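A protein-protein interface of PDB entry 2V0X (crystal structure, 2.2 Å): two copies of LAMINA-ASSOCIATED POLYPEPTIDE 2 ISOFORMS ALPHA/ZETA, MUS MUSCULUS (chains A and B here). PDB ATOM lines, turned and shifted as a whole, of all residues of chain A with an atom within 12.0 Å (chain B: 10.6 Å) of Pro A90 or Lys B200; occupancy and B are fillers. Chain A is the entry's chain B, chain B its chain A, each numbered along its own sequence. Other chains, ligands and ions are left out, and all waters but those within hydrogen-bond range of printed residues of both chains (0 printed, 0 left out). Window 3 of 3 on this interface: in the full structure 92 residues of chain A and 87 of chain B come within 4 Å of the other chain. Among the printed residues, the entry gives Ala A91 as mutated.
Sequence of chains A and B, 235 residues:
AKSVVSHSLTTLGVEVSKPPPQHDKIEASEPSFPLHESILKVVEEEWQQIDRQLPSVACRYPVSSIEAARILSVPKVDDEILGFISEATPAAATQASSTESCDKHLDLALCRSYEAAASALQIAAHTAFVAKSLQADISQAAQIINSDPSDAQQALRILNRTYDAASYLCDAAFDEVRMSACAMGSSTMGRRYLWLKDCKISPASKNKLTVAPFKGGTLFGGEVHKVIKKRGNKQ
The side-chain hydroxyl of Thr A99 sits at hydrogen-bond distance from the side-chain amino group of Lys B197 (3.2 Å).
The side-chain amino group (NZ) of Lys B197 is in salt-bridge range of the side-chain carboxylate (OD2) of Asp A103 (3.7 Å).
N of Lys B200 lies within hydrogen-bond range of O of Ala A88 (2.7 Å).
Of the printed residues of chain B, Phe A84 touches Ile B201.
Printed residues of chain B within 4 Å of Ile A85: Trp B195 (3.5 Å), Leu B196 (3.8 Å) and Cys B199 (3.5 Å).
Of chain B, only Cys B199 (3.6 Å) comes within 4 Å of Thr A89.
Pro A90 touches one residue of chain B.
No residue of chain B comes within 4 Å of Ala A91.
Ala A92 touches none of the printed residues of chain B.
Thr A94 touches none of the printed residues of chain B.
Printed residues of chain A within 4 Å of Trp B195: Ile A85 (3.5 Å).
Printed residues of chain A within 4 Å of Lys B197: Thr A99 (3.2 Å) and Asp A103 (3.2 Å).
Cys B199 touches three residues of chain A.
Of chain A, only Ala A88 and Pro A90 come within 4 Å of Lys B200.
Of the printed residues of chain A, Ile B201 touches Phe A84 (3.5 Å) and Ala A88 (3.98 Å).
No residue of chain A comes within 4 Å of Ser B202.
The nearest residue of chain B that does not touch Pro A90 is Asp B198 (4.1 Å).
The nearest residue of chain A that does not touch Lys B200 is Thr A89 (4.7 Å).
The nearest printed residue of chain A that does not touch Leu B196 is Ile A81 (5.5 Å).
Positions printed for both chains: 98 and 99.
Of the 14 pairs that touch across the chains among the printed residues, none has its exchanged pair printed and touching as well.
Among the printed residues, merely in contact across the chains: Phe A84 with Ile B201, Ile A85 with Trp B195, Ile A85 with Leu B196, Ile A85 with Cys B199, Ala A88 with Cys B199, Ala A88 with Ile B201, Thr A89 with Cys B199, Pro A90 with Lys B200, Thr A99 with Asp B198, Asp A103 with Leu B194 and Asp A103 with Asp B198.
Of the 21 printed residues of chain A, 7 touch a printed residue of chain B.
Printed residues of chain A that touch a printed residue of chain B: Phe A84, Ile A85, Ala A88, Thr A89, Pro A90, Thr A99 and Asp A103.
Hydrophobic or aromatic side chains of chain A within 4 Å of the printed part of chain B: Phe A84, Ile A85, Ala A88 and Pro A90.
Among the printed residues, Asp or Glu carboxylates within 4 Å of a Lys or Arg side-chain nitrogen of the other chain: Asp A103 with Lys B197 (3.7 Å).
The side-chain sulfur (SG) of Cys B199 is in hydrogen-bond range of the backbone carbonyl oxygen (O) of Leu B196 (3.6 Å).
NZ of Lys B206 sits at hydrogen-bond distance from O of Leu B196.
NZ of Lys B197 lies within salt-bridge range of OD1 of Asp B198, 3.0 Å away.
O of Cys B199 is in hydrogen-bond range of NZ of Lys B206 (3.1 Å).
O of Ile A85 is in hydrogen-bond range of OG1 of Thr A89 (2.7 Å).
The side-chain hydroxyl of Thr A99 sits at hydrogen-bond distance from the side-chain carboxylate of Asp A103, at 2.8 Å.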
ATOM      1  N   ILE A  81      -7.962   2.714  13.768  1.00  0.00           N
ATOM      2  CA  ILE A  81      -8.816   3.504  12.888  1.00  0.00           C
ATOM      3  C   ILE A  81      -8.010   4.706  12.391  1.00  0.00           C
ATOM      4  O   ILE A  81      -8.089   5.074  11.227  1.00  0.00           O
ATOM      5  CB  ILE A  81     -10.100   3.996  13.616  1.00  0.00           C
ATOM      6  CG1 ILE A  81     -10.873   2.809  14.197  1.00  0.00           C
ATOM      7  CG2 ILE A  81     -10.992   4.771  12.656  1.00  0.00           C
ATOM      8  CD1 ILE A  81     -11.344   1.798  13.164  1.00  0.00           C
ATOM      9  N   LEU A  82      -7.222   5.290  13.285  1.00  0.00           N
ATOM     10  CA  LEU A  82      -6.385   6.447  12.980  1.00  0.00           C
ATOM     11  C   LEU A  82      -5.302   6.061  11.971  1.00  0.00           C
ATOM     12  O   LEU A  82      -4.989   6.822  11.048  1.00  0.00           O
ATOM     13  CB  LEU A  82      -5.732   6.970  14.262  1.00  0.00           C
ATOM     14  CG  LEU A  82      -5.915   8.456  14.552  1.00  0.00           C
ATOM     15  CD1 LEU A  82      -5.208   8.816  15.860  1.00  0.00           C
ATOM     16  CD2 LEU A  82      -5.373   9.282  13.386  1.00  0.00           C
ATOM     17  N   GLY A  83      -4.741   4.871  12.167  1.00  0.00           N
ATOM     18  CA  GLY A  83      -3.718   4.357  11.279  1.00  0.00           C
ATOM     19  C   GLY A  83      -4.332   4.127   9.922  1.00  0.00           C
ATOM     20  O   GLY A  83      -3.762   4.524   8.905  1.00  0.00           O
ATOM     21  N   PHE A  84      -5.526   3.547   9.909  1.00  0.00           N
ATOM     22  CA  PHE A  84      -6.232   3.281   8.663  1.00  0.00           C
ATOM     23  C   PHE A  84      -6.566   4.579   7.913  1.00  0.00           C
ATOM     24  O   PHE A  84      -6.401   4.663   6.695  1.00  0.00           O
ATOM     25  CB  PHE A  84      -7.516   2.490   8.932  1.00  0.00           C
ATOM     26  CG  PHE A  84      -8.221   2.030   7.683  1.00  0.00           C
ATOM     27  CD1 PHE A  84      -7.670   1.025   6.888  1.00  0.00           C
ATOM     28  CD2 PHE A  84      -9.430   2.601   7.300  1.00  0.00           C
ATOM     29  CE1 PHE A  84      -8.317   0.594   5.726  1.00  0.00           C
ATOM     30  CE2 PHE A  84     -10.088   2.179   6.140  1.00  0.00           C
ATOM     31  CZ  PHE A  84      -9.528   1.172   5.350  1.00  0.00           C
ATOM     32  N   ILE A  85      -7.057   5.575   8.641  1.00  0.00           N
ATOM     33  CA  ILE A  85      -7.413   6.861   8.052  1.00  0.00           C
ATOM     34  C   ILE A  85      -6.172   7.514   7.438  1.00  0.00           C
ATOM     35  O   ILE A  85      -6.219   8.003   6.315  1.00  0.00           O
ATOM     36  CB  ILE A  85      -8.033   7.832   9.108  1.00  0.00           C
ATOM     37  CG1 ILE A  85      -9.366   7.272   9.626  1.00  0.00           C
ATOM     38  CG2 ILE A  85      -8.221   9.228   8.510  1.00  0.00           C
ATOM     39  CD1 ILE A  85     -10.077   8.177  10.633  1.00  0.00           C
ATOM     40  N   SER A  86      -5.069   7.491   8.180  1.00  0.00           N
ATOM     41  CA  SER A  86      -3.813   8.082   7.730  1.00  0.00           C
ATOM     42  C   SER A  86      -3.324   7.428   6.438  1.00  0.00           C
ATOM     43  O   SER A  86      -3.005   8.121   5.472  1.00  0.00           O
ATOM     44  CB  SER A  86      -2.749   7.960   8.822  1.00  0.00           C
ATOM     45  OG  SER A  86      -1.629   8.789   8.546  1.00  0.00           O
ATOM     46  N   GLU A  87      -3.299   6.098   6.413  1.00  0.00           N
ATOM     47  CA  GLU A  87      -2.850   5.358   5.233  1.00  0.00           C
ATOM     48  C   GLU A  87      -3.748   5.635   4.030  1.00  0.00           C
ATOM     49  O   GLU A  87      -3.306   5.586   2.889  1.00  0.00           O
ATOM     50  CB  GLU A  87      -2.775   3.858   5.532  1.00  0.00           C
ATOM     51  CG  GLU A  87      -1.699   3.516   6.542  1.00  0.00           C
ATOM     52  CD  GLU A  87      -1.674   2.052   6.912  1.00  0.00           C
ATOM     53  OE1 GLU A  87      -0.623   1.409   6.704  1.00  0.00           O
ATOM     54  OE2 GLU A  87      -2.697   1.545   7.423  1.00  0.00           O
ATOM     55  N   ALA A  88      -5.005   5.969   4.292  1.00  0.00           N
ATOM     56  CA  ALA A  88      -5.936   6.293   3.222  1.00  0.00           C
ATOM     57  C   ALA A  88      -5.924   7.808   2.926  1.00  0.00           C
ATOM     58  O   ALA A  88      -6.732   8.298   2.144  1.00  0.00           O
ATOM     59  CB  ALA A  88      -7.345   5.817   3.583  1.00  0.00           C
ATOM     60  N   THR A  89      -5.017   8.556   3.550  1.00  0.00           N
ATOM     61  CA  THR A  89      -4.935   9.999   3.302  1.00  0.00           C
ATOM     62  C   THR A  89      -3.760  10.327   2.378  1.00  0.00           C
ATOM     63  O   THR A  89      -2.595  10.195   2.762  1.00  0.00           O
ATOM     64  CB  THR A  89      -4.809  10.807   4.626  1.00  0.00           C
ATOM     65  OG1 THR A  89      -5.926  10.512   5.467  1.00  0.00           O
ATOM     66  CG2 THR A  89      -4.763  12.317   4.348  1.00  0.00           C
ATOM     67  N   PRO A  90      -4.055  10.728   1.129  1.00  0.00           N
ATOM     68  CA  PRO A  90      -3.036  11.076   0.129  1.00  0.00           C
ATOM     69  C   PRO A  90      -2.270  12.339   0.519  1.00  0.00           C
ATOM     70  O   PRO A  90      -2.821  13.231   1.155  1.00  0.00           O
ATOM     71  CB  PRO A  90      -3.870  11.324  -1.136  1.00  0.00           C
ATOM     72  CG  PRO A  90      -5.139  10.555  -0.888  1.00  0.00           C
ATOM     73  CD  PRO A  90      -5.403  10.858   0.555  1.00  0.00           C
ATOM     74  N   ALA A  91      -1.008  12.415   0.112  1.00  0.00           N
ATOM     75  CA  ALA A  91      -0.165  13.566   0.409  1.00  0.00           C
ATOM     76  C   ALA A  91       0.685  13.918  -0.805  1.00  0.00           C
ATOM     77  O   ALA A  91       1.169  13.052  -1.531  1.00  0.00           O
ATOM     78  CB  ALA A  91       0.713  13.280   1.613  1.00  0.00           C
ATOM     79  N   ALA A  92       0.873  15.215  -1.019  1.00  0.00           N
ATOM     80  CA  ALA A  92       1.663  15.740  -2.129  1.00  0.00           C
ATOM     81  C   ALA A  92       1.727  17.256  -1.949  1.00  0.00           C
ATOM     82  O   ALA A  92       1.338  17.769  -0.907  1.00  0.00           O
ATOM     83  CB  ALA A  92       1.049  15.370  -3.471  1.00  0.00           C
ATOM     84  N   ALA A  93       2.214  17.964  -2.961  1.00  0.00           N
ATOM     85  CA  ALA A  93       2.291  19.416  -2.878  1.00  0.00           C
ATOM     86  C   ALA A  93       0.924  20.019  -3.187  1.00  0.00           C
ATOM     87  O   ALA A  93       0.150  20.333  -2.276  1.00  0.00           O
ATOM     88  CB  ALA A  93       3.354  19.945  -3.826  1.00  0.00           C
ATOM     89  N   THR A  94       0.656  20.174  -4.481  1.00  0.00           N
ATOM     90  CA  THR A  94      -0.586  20.728  -5.016  1.00  0.00           C
ATOM     91  C   THR A  94      -1.453  21.581  -4.082  1.00  0.00           C
ATOM     92  O   THR A  94      -1.109  22.734  -3.805  1.00  0.00           O
ATOM     93  CB  THR A  94      -1.432  19.629  -5.713  1.00  0.00           C
ATOM     94  OG1 THR A  94      -1.658  18.540  -4.807  1.00  0.00           O
ATOM     95  CG2 THR A  94      -0.706  19.111  -6.954  1.00  0.00           C
ATOM     96  N   GLN A  95      -2.544  20.997  -3.584  1.00  0.00           N
ATOM     97  CA  GLN A  95      -3.504  21.664  -2.700  1.00  0.00           C
ATOM     98  C   GLN A  95      -2.971  22.838  -1.878  1.00  0.00           C
ATOM     99  O   GLN A  95      -3.401  23.975  -2.073  1.00  0.00           O
ATOM    100  CB  GLN A  95      -4.064  20.676  -1.677  1.00  0.00           C
ATOM    101  CG  GLN A  95      -4.792  19.493  -2.291  1.00  0.00           C
ATOM    102  CD  GLN A  95      -5.333  18.536  -1.247  1.00  0.00           C
ATOM    103  OE1 GLN A  95      -5.167  18.753  -0.047  1.00  0.00           O
ATOM    104  NE2 GLN A  95      -6.009  17.418  -1.478  1.00  0.00           N
ATOM    105  N   ALA A  96      -2.067  22.551  -0.943  1.00  0.00           N
ATOM    106  CA  ALA A  96      -1.464  23.566  -0.069  1.00  0.00           C
ATOM    107  C   ALA A  96      -2.431  24.193   0.938  1.00  0.00           C
ATOM    108  O   ALA A  96      -2.017  24.627   2.011  1.00  0.00           O
ATOM    109  CB  ALA A  96      -0.775  24.653  -0.897  1.00  0.00           C
ATOM    110  N   SER A  97      -3.713  24.246   0.591  1.00  0.00           N
ATOM    111  CA  SER A  97      -4.728  24.814   1.467  1.00  0.00           C
ATOM    112  C   SER A  97      -5.118  23.822   2.558  1.00  0.00           C
ATOM    113  O   SER A  97      -6.191  23.215   2.499  1.00  0.00           O
ATOM    114  CB  SER A  97      -5.960  25.201   0.642  1.00  0.00           C
ATOM    115  OG  SER A  97      -6.451  24.092  -0.095  1.00  0.00           O
ATOM    116  N   SER A  98      -4.236  23.627   3.536  1.00  0.00           N
ATOM    117  CA  SER A  98      -4.525  22.701   4.622  1.00  0.00           C
ATOM    118  C   SER A  98      -5.598  23.270   5.549  1.00  0.00           C
ATOM    119  O   SER A  98      -5.452  24.365   6.100  1.00  0.00           O
ATOM    120  CB  SER A  98      -3.252  22.346   5.405  1.00  0.00           C
ATOM    121  OG  SER A  98      -2.642  23.485   5.983  1.00  0.00           O
ATOM    122  N   THR A  99      -6.695  22.531   5.687  1.00  0.00           N
ATOM    123  CA  THR A  99      -7.800  22.943   6.543  1.00  0.00           C
ATOM    124  C   THR A  99      -7.488  22.674   8.012  1.00  0.00           C
ATOM    125  O   THR A  99      -8.288  22.998   8.889  1.00  0.00           O
ATOM    126  CB  THR A  99      -9.091  22.199   6.166  1.00  0.00           C
ATOM    127  OG1 THR A  99      -8.825  20.792   6.090  1.00  0.00           O
ATOM    128  CG2 THR A  99      -9.614  22.687   4.824  1.00  0.00           C
ATOM    129  N   GLU A 100      -6.316  22.092   8.261  1.00  0.00           N
ATOM    130  CA  GLU A 100      -5.840  21.742   9.599  1.00  0.00           C
ATOM    131  C   GLU A 100      -6.291  22.698  10.700  1.00  0.00           C
ATOM    132  O   GLU A 100      -6.793  22.262  11.734  1.00  0.00           O
ATOM    133  CB  GLU A 100      -4.314  21.648   9.595  1.00  0.00           C
ATOM    134  CG  GLU A 100      -3.703  21.286  10.940  1.00  0.00           C
ATOM    135  CD  GLU A 100      -2.221  21.602  11.002  1.00  0.00           C
ATOM    136  OE1 GLU A 100      -1.873  22.767  11.296  1.00  0.00           O
ATOM    137  OE2 GLU A 100      -1.405  20.690  10.753  1.00  0.00           O
ATOM    138  N   ASP A 103     -10.086  22.605  11.043  1.00  0.00           N
ATOM    139  CA  ASP A 103     -10.379  21.274  11.548  1.00  0.00           C
ATOM    140  C   ASP A 103     -10.116  21.155  13.055  1.00  0.00           C
ATOM    141  O   ASP A 103     -10.941  20.618  13.781  1.00  0.00           O
ATOM    142  CB  ASP A 103      -9.592  20.216  10.765  1.00  0.00           C
ATOM    143  CG  ASP A 103      -9.997  20.152   9.288  1.00  0.00           C
ATOM    144  OD1 ASP A 103     -11.009  20.789   8.901  1.00  0.00           O
ATOM    145  OD2 ASP A 103      -9.293  19.466   8.511  1.00  0.00           O
ATOM    146  N   SER B  98     -14.536  18.667  -2.250  1.00  0.00           N
ATOM    147  CA  SER B  98     -15.981  18.470  -2.299  1.00  0.00           C
ATOM    148  C   SER B  98     -16.526  18.190  -0.895  1.00  0.00           C
ATOM    149  O   SER B  98     -17.514  17.472  -0.720  1.00  0.00           O
ATOM    150  CB  SER B  98     -16.318  17.316  -3.251  1.00  0.00           C
ATOM    151  OG  SER B  98     -15.786  17.559  -4.546  1.00  0.00           O
ATOM    152  N   THR B  99     -15.905  18.819   0.098  1.00  0.00           N
ATOM    153  CA  THR B  99     -16.294  18.651   1.492  1.00  0.00           C
ATOM    154  C   THR B  99     -17.597  19.358   1.886  1.00  0.00           C
ATOM    155  O   THR B  99     -17.900  19.481   3.076  1.00  0.00           O
ATOM    156  CB  THR B  99     -15.160  19.125   2.429  1.00  0.00           C
ATOM    157  OG1 THR B  99     -14.694  20.413   2.001  1.00  0.00           O
ATOM    158  CG2 THR B  99     -13.999  18.132   2.417  1.00  0.00           C
ATOM    159  N   SER B 101     -20.535  18.265   1.583  1.00  0.00           N
ATOM    160  CA  SER B 101     -21.368  17.269   2.243  1.00  0.00           C
ATOM    161  C   SER B 101     -20.952  17.239   3.716  1.00  0.00           C
ATOM    162  O   SER B 101     -21.798  17.212   4.609  1.00  0.00           O
ATOM    163  CB  SER B 101     -21.159  15.897   1.595  1.00  0.00           C
ATOM    164  OG  SER B 101     -19.776  15.606   1.451  1.00  0.00           O
ATOM    165  N   TYR B 193     -17.623  12.466  11.174  1.00  0.00           N
ATOM    166  CA  TYR B 193     -17.579  13.053   9.833  1.00  0.00           C
ATOM    167  C   TYR B 193     -16.282  13.812   9.663  1.00  0.00           C
ATOM    168  O   TYR B 193     -15.578  13.639   8.664  1.00  0.00           O
ATOM    169  CB  TYR B 193     -18.730  14.027   9.619  1.00  0.00           C
ATOM    170  CG  TYR B 193     -20.019  13.356   9.238  1.00  0.00           C
ATOM    171  CD1 TYR B 193     -21.097  13.316  10.130  1.00  0.00           C
ATOM    172  CD2 TYR B 193     -20.176  12.779   7.978  1.00  0.00           C
ATOM    173  CE1 TYR B 193     -22.304  12.721   9.776  1.00  0.00           C
ATOM    174  CE2 TYR B 193     -21.381  12.174   7.609  1.00  0.00           C
ATOM    175  CZ  TYR B 193     -22.441  12.151   8.514  1.00  0.00           C
ATOM    176  OH  TYR B 193     -23.634  11.566   8.161  1.00  0.00           O
ATOM    177  N   LEU B 194     -15.936  14.613  10.670  1.00  0.00           N
ATOM    178  CA  LEU B 194     -14.712  15.412  10.606  1.00  0.00           C
ATOM    179  C   LEU B 194     -13.432  14.585  10.395  1.00  0.00           C
ATOM    180  O   LEU B 194     -12.594  14.931   9.562  1.00  0.00           O
ATOM    181  CB  LEU B 194     -14.560  16.276  11.852  1.00  0.00           C
ATOM    182  CG  LEU B 194     -13.404  17.277  11.849  1.00  0.00           C
ATOM    183  CD1 LEU B 194     -13.617  18.350  10.773  1.00  0.00           C
ATOM    184  CD2 LEU B 194     -13.294  17.934  13.214  1.00  0.00           C
ATOM    185  N   TRP B 195     -13.301  13.475  11.108  1.00  0.00           N
ATOM    186  CA  TRP B 195     -12.101  12.652  10.992  1.00  0.00           C
ATOM    187  C   TRP B 195     -11.999  11.816   9.708  1.00  0.00           C
ATOM    188  O   TRP B 195     -10.907  11.384   9.341  1.00  0.00           O
ATOM    189  CB  TRP B 195     -11.932  11.767  12.242  1.00  0.00           C
ATOM    190  CG  TRP B 195     -11.399  12.534  13.410  1.00  0.00           C
ATOM    191  CD1 TRP B 195     -12.120  13.285  14.308  1.00  0.00           C
ATOM    192  CD2 TRP B 195     -10.024  12.714  13.751  1.00  0.00           C
ATOM    193  NE1 TRP B 195     -11.270  13.937  15.171  1.00  0.00           N
ATOM    194  CE2 TRP B 195      -9.977  13.603  14.852  1.00  0.00           C
ATOM    195  CE3 TRP B 195      -8.819  12.218  13.226  1.00  0.00           C
ATOM    196  CZ2 TRP B 195      -8.765  14.007  15.439  1.00  0.00           C
ATOM    197  CZ3 TRP B 195      -7.619  12.615  13.805  1.00  0.00           C
ATOM    198  CH2 TRP B 195      -7.601  13.503  14.902  1.00  0.00           C
ATOM    199  N   LEU B 196     -13.128  11.612   9.032  1.00  0.00           N
ATOM    200  CA  LEU B 196     -13.180  10.849   7.789  1.00  0.00           C
ATOM    201  C   LEU B 196     -13.219  11.731   6.537  1.00  0.00           C
ATOM    202  O   LEU B 196     -13.134  11.220   5.427  1.00  0.00           O
ATOM    203  CB  LEU B 196     -14.443   9.992   7.766  1.00  0.00           C
ATOM    204  CG  LEU B 196     -14.604   8.948   8.874  1.00  0.00           C
ATOM    205  CD1 LEU B 196     -15.928   8.208   8.706  1.00  0.00           C
ATOM    206  CD2 LEU B 196     -13.423   7.986   8.844  1.00  0.00           C
ATOM    207  N   LYS B 197     -13.332  13.046   6.708  1.00  0.00           N
ATOM    208  CA  LYS B 197     -13.468  13.945   5.569  1.00  0.00           C
ATOM    209  C   LYS B 197     -12.351  14.009   4.525  1.00  0.00           C
ATOM    210  O   LYS B 197     -12.625  14.325   3.364  1.00  0.00           O
ATOM    211  CB  LYS B 197     -13.807  15.363   6.038  1.00  0.00           C
ATOM    212  CG  LYS B 197     -12.603  16.239   6.331  1.00  0.00           C
ATOM    213  CD  LYS B 197     -13.027  17.654   6.671  1.00  0.00           C
ATOM    214  CE  LYS B 197     -11.842  18.592   6.719  1.00  0.00           C
ATOM    215  NZ  LYS B 197     -11.237  18.811   5.380  1.00  0.00           N
ATOM    216  N   ASP B 198     -11.111  13.729   4.918  1.00  0.00           N
ATOM    217  CA  ASP B 198      -9.994  13.814   3.975  1.00  0.00           C
ATOM    218  C   ASP B 198      -9.376  12.507   3.491  1.00  0.00           C
ATOM    219  O   ASP B 198      -8.576  12.518   2.555  1.00  0.00           O
ATOM    220  CB  ASP B 198      -8.898  14.739   4.516  1.00  0.00           C
ATOM    221  CG  ASP B 198      -9.332  16.201   4.560  1.00  0.00           C
ATOM    222  OD1 ASP B 198      -8.956  16.906   5.520  1.00  0.00           O
ATOM    223  OD2 ASP B 198     -10.054  16.644   3.637  1.00  0.00           O
ATOM    224  N   CYS B 199      -9.705  11.390   4.130  1.00  0.00           N
ATOM    225  CA  CYS B 199      -9.149  10.122   3.700  1.00  0.00           C
ATOM    226  C   CYS B 199      -9.934   9.604   2.490  1.00  0.00           C
ATOM    227  O   CYS B 199     -11.049  10.057   2.212  1.00  0.00           O
ATOM    228  CB  CYS B 199      -9.152   9.104   4.840  1.00  0.00           C
ATOM    229  SG  CYS B 199     -10.767   8.529   5.306  1.00  0.00           S
ATOM    230  N   LYS B 200      -9.337   8.669   1.761  1.00  0.00           N
ATOM    231  CA  LYS B 200      -9.957   8.114   0.573  1.00  0.00           C
ATOM    232  C   LYS B 200     -10.504   6.716   0.769  1.00  0.00           C
ATOM    233  O   LYS B 200      -9.799   5.721   0.581  1.00  0.00           O
ATOM    234  CB  LYS B 200      -8.983   8.147  -0.606  1.00  0.00           C
ATOM    235  CG  LYS B 200      -8.822   9.531  -1.213  1.00  0.00           C
ATOM    236  CD  LYS B 200     -10.174  10.101  -1.647  1.00  0.00           C
ATOM    237  CE  LYS B 200     -10.869   9.203  -2.672  1.00  0.00           C
ATOM    238  NZ  LYS B 200     -12.257   9.658  -2.965  1.00  0.00           N
ATOM    239  N   ILE B 201     -11.764   6.658   1.185  1.00  0.00           N
ATOM    240  CA  ILE B 201     -12.464   5.402   1.406  1.00  0.00           C
ATOM    241  C   ILE B 201     -13.850   5.598   0.798  1.00  0.00           C
ATOM    242  O   ILE B 201     -14.354   6.723   0.733  1.00  0.00           O
ATOM    243  CB  ILE B 201     -12.606   5.071   2.910  1.00  0.00           C
ATOM    244  CG1 ILE B 201     -11.304   5.375   3.655  1.00  0.00           C
ATOM    245  CG2 ILE B 201     -12.915   3.589   3.077  1.00  0.00           C
ATOM    246  CD1 ILE B 201     -11.425   5.274   5.170  1.00  0.00           C
ATOM    247  N   SER B 202     -14.448   4.511   0.320  1.00  0.00           N
ATOM    248  CA  SER B 202     -15.767   4.577  -0.299  1.00  0.00           C
ATOM    249  C   SER B 202     -16.814   5.173   0.632  1.00  0.00           C
ATOM    250  O   SER B 202     -16.776   4.941   1.846  1.00  0.00           O
ATOM    251  CB  SER B 202     -16.204   3.179  -0.749  1.00  0.00           C
ATOM    252  OG  SER B 202     -15.879   2.197   0.222  1.00  0.00           O
ATOM    253  N   PRO B 203     -17.775   5.937   0.075  1.00  0.00           N
ATOM    254  CA  PRO B 203     -18.842   6.562   0.868  1.00  0.00           C
ATOM    255  C   PRO B 203     -19.562   5.507   1.703  1.00  0.00           C
ATOM    256  O   PRO B 203     -20.085   5.804   2.772  1.00  0.00           O
ATOM    257  CB  PRO B 203     -19.763   7.140  -0.203  1.00  0.00           C
ATOM    258  CG  PRO B 203     -18.805   7.521  -1.282  1.00  0.00           C
ATOM    259  CD  PRO B 203     -17.895   6.313  -1.344  1.00  0.00           C
ATOM    260  N   ALA B 204     -19.566   4.273   1.205  1.00  0.00           N
ATOM    261  CA  ALA B 204     -20.200   3.151   1.889  1.00  0.00           C
ATOM    262  C   ALA B 204     -19.511   2.882   3.225  1.00  0.00           C
ATOM    263  O   ALA B 204     -20.157   2.840   4.272  1.00  0.00           O
ATOM    264  CB  ALA B 204     -20.148   1.903   1.010  1.00  0.00           C
ATOM    265  N   SER B 205     -18.192   2.724   3.181  1.00  0.00           N
ATOM    266  CA  SER B 205     -17.403   2.465   4.378  1.00  0.00           C
ATOM    267  C   SER B 205     -17.483   3.640   5.354  1.00  0.00           C
ATOM    268  O   SER B 205     -17.583   3.440   6.566  1.00  0.00           O
ATOM    269  CB  SER B 205     -15.949   2.202   3.991  1.00  0.00           C
ATOM    270  OG  SER B 205     -15.874   1.263   2.934  1.00  0.00           O
ATOM    271  N   LYS B 206     -17.442   4.860   4.822  1.00  0.00           N
ATOM    272  CA  LYS B 206     -17.527   6.058   5.653  1.00  0.00           C
ATOM    273  C   LYS B 206     -18.887   6.142   6.338  1.00  0.00           C
ATOM    274  O   LYS B 206     -18.969   6.400   7.541  1.00  0.00           O
ATOM    275  CB  LYS B 206     -17.287   7.327   4.827  1.00  0.00           C
ATOM    276  CG  LYS B 206     -15.839   7.568   4.433  1.00  0.00           C
ATOM    277  CD  LYS B 206     -15.678   8.937   3.787  1.00  0.00           C
ATOM    278  CE  LYS B 206     -14.246   9.184   3.341  1.00  0.00           C
ATOM    279  NZ  LYS B 206     -14.068  10.570   2.825  1.00  0.00           N
ATOM    280  N   LEU B 209     -19.252   3.584   9.130  1.00  0.00           N
ATOM    281  CA  LEU B 209     -18.501   4.039  10.295  1.00  0.00           C
ATOM    282  C   LEU B 209     -19.170   5.191  11.050  1.00  0.00           C
ATOM    283  O   LEU B 209     -19.095   5.263  12.272  1.00  0.00           O
ATOM    284  CB  LEU B 209     -17.084   4.440   9.877  1.00  0.00           C
ATOM    285  CG  LEU B 209     -16.084   3.295   9.674  1.00  0.00           C
ATOM    286  CD1 LEU B 209     -14.910   3.757   8.838  1.00  0.00           C
ATOM    287  CD2 LEU B 209     -15.604   2.766  11.025  1.00  0.00           C
ATOM    288  N   VAL B 227     -12.475  -3.475   5.979  1.00  0.00           N
ATOM    289  CA  VAL B 227     -12.474  -3.926   4.589  1.00  0.00           C
ATOM    290  C   VAL B 227     -13.587  -4.949   4.367  1.00  0.00           C
ATOM    291  O   VAL B 227     -13.844  -5.794   5.226  1.00  0.00           O
ATOM    292  CB  VAL B 227     -11.112  -4.564   4.209  1.00  0.00           C
ATOM    293  CG1 VAL B 227     -11.131  -5.038   2.761  1.00  0.00           C
ATOM    294  CG2 VAL B 227      -9.981  -3.566   4.427  1.00  0.00           C
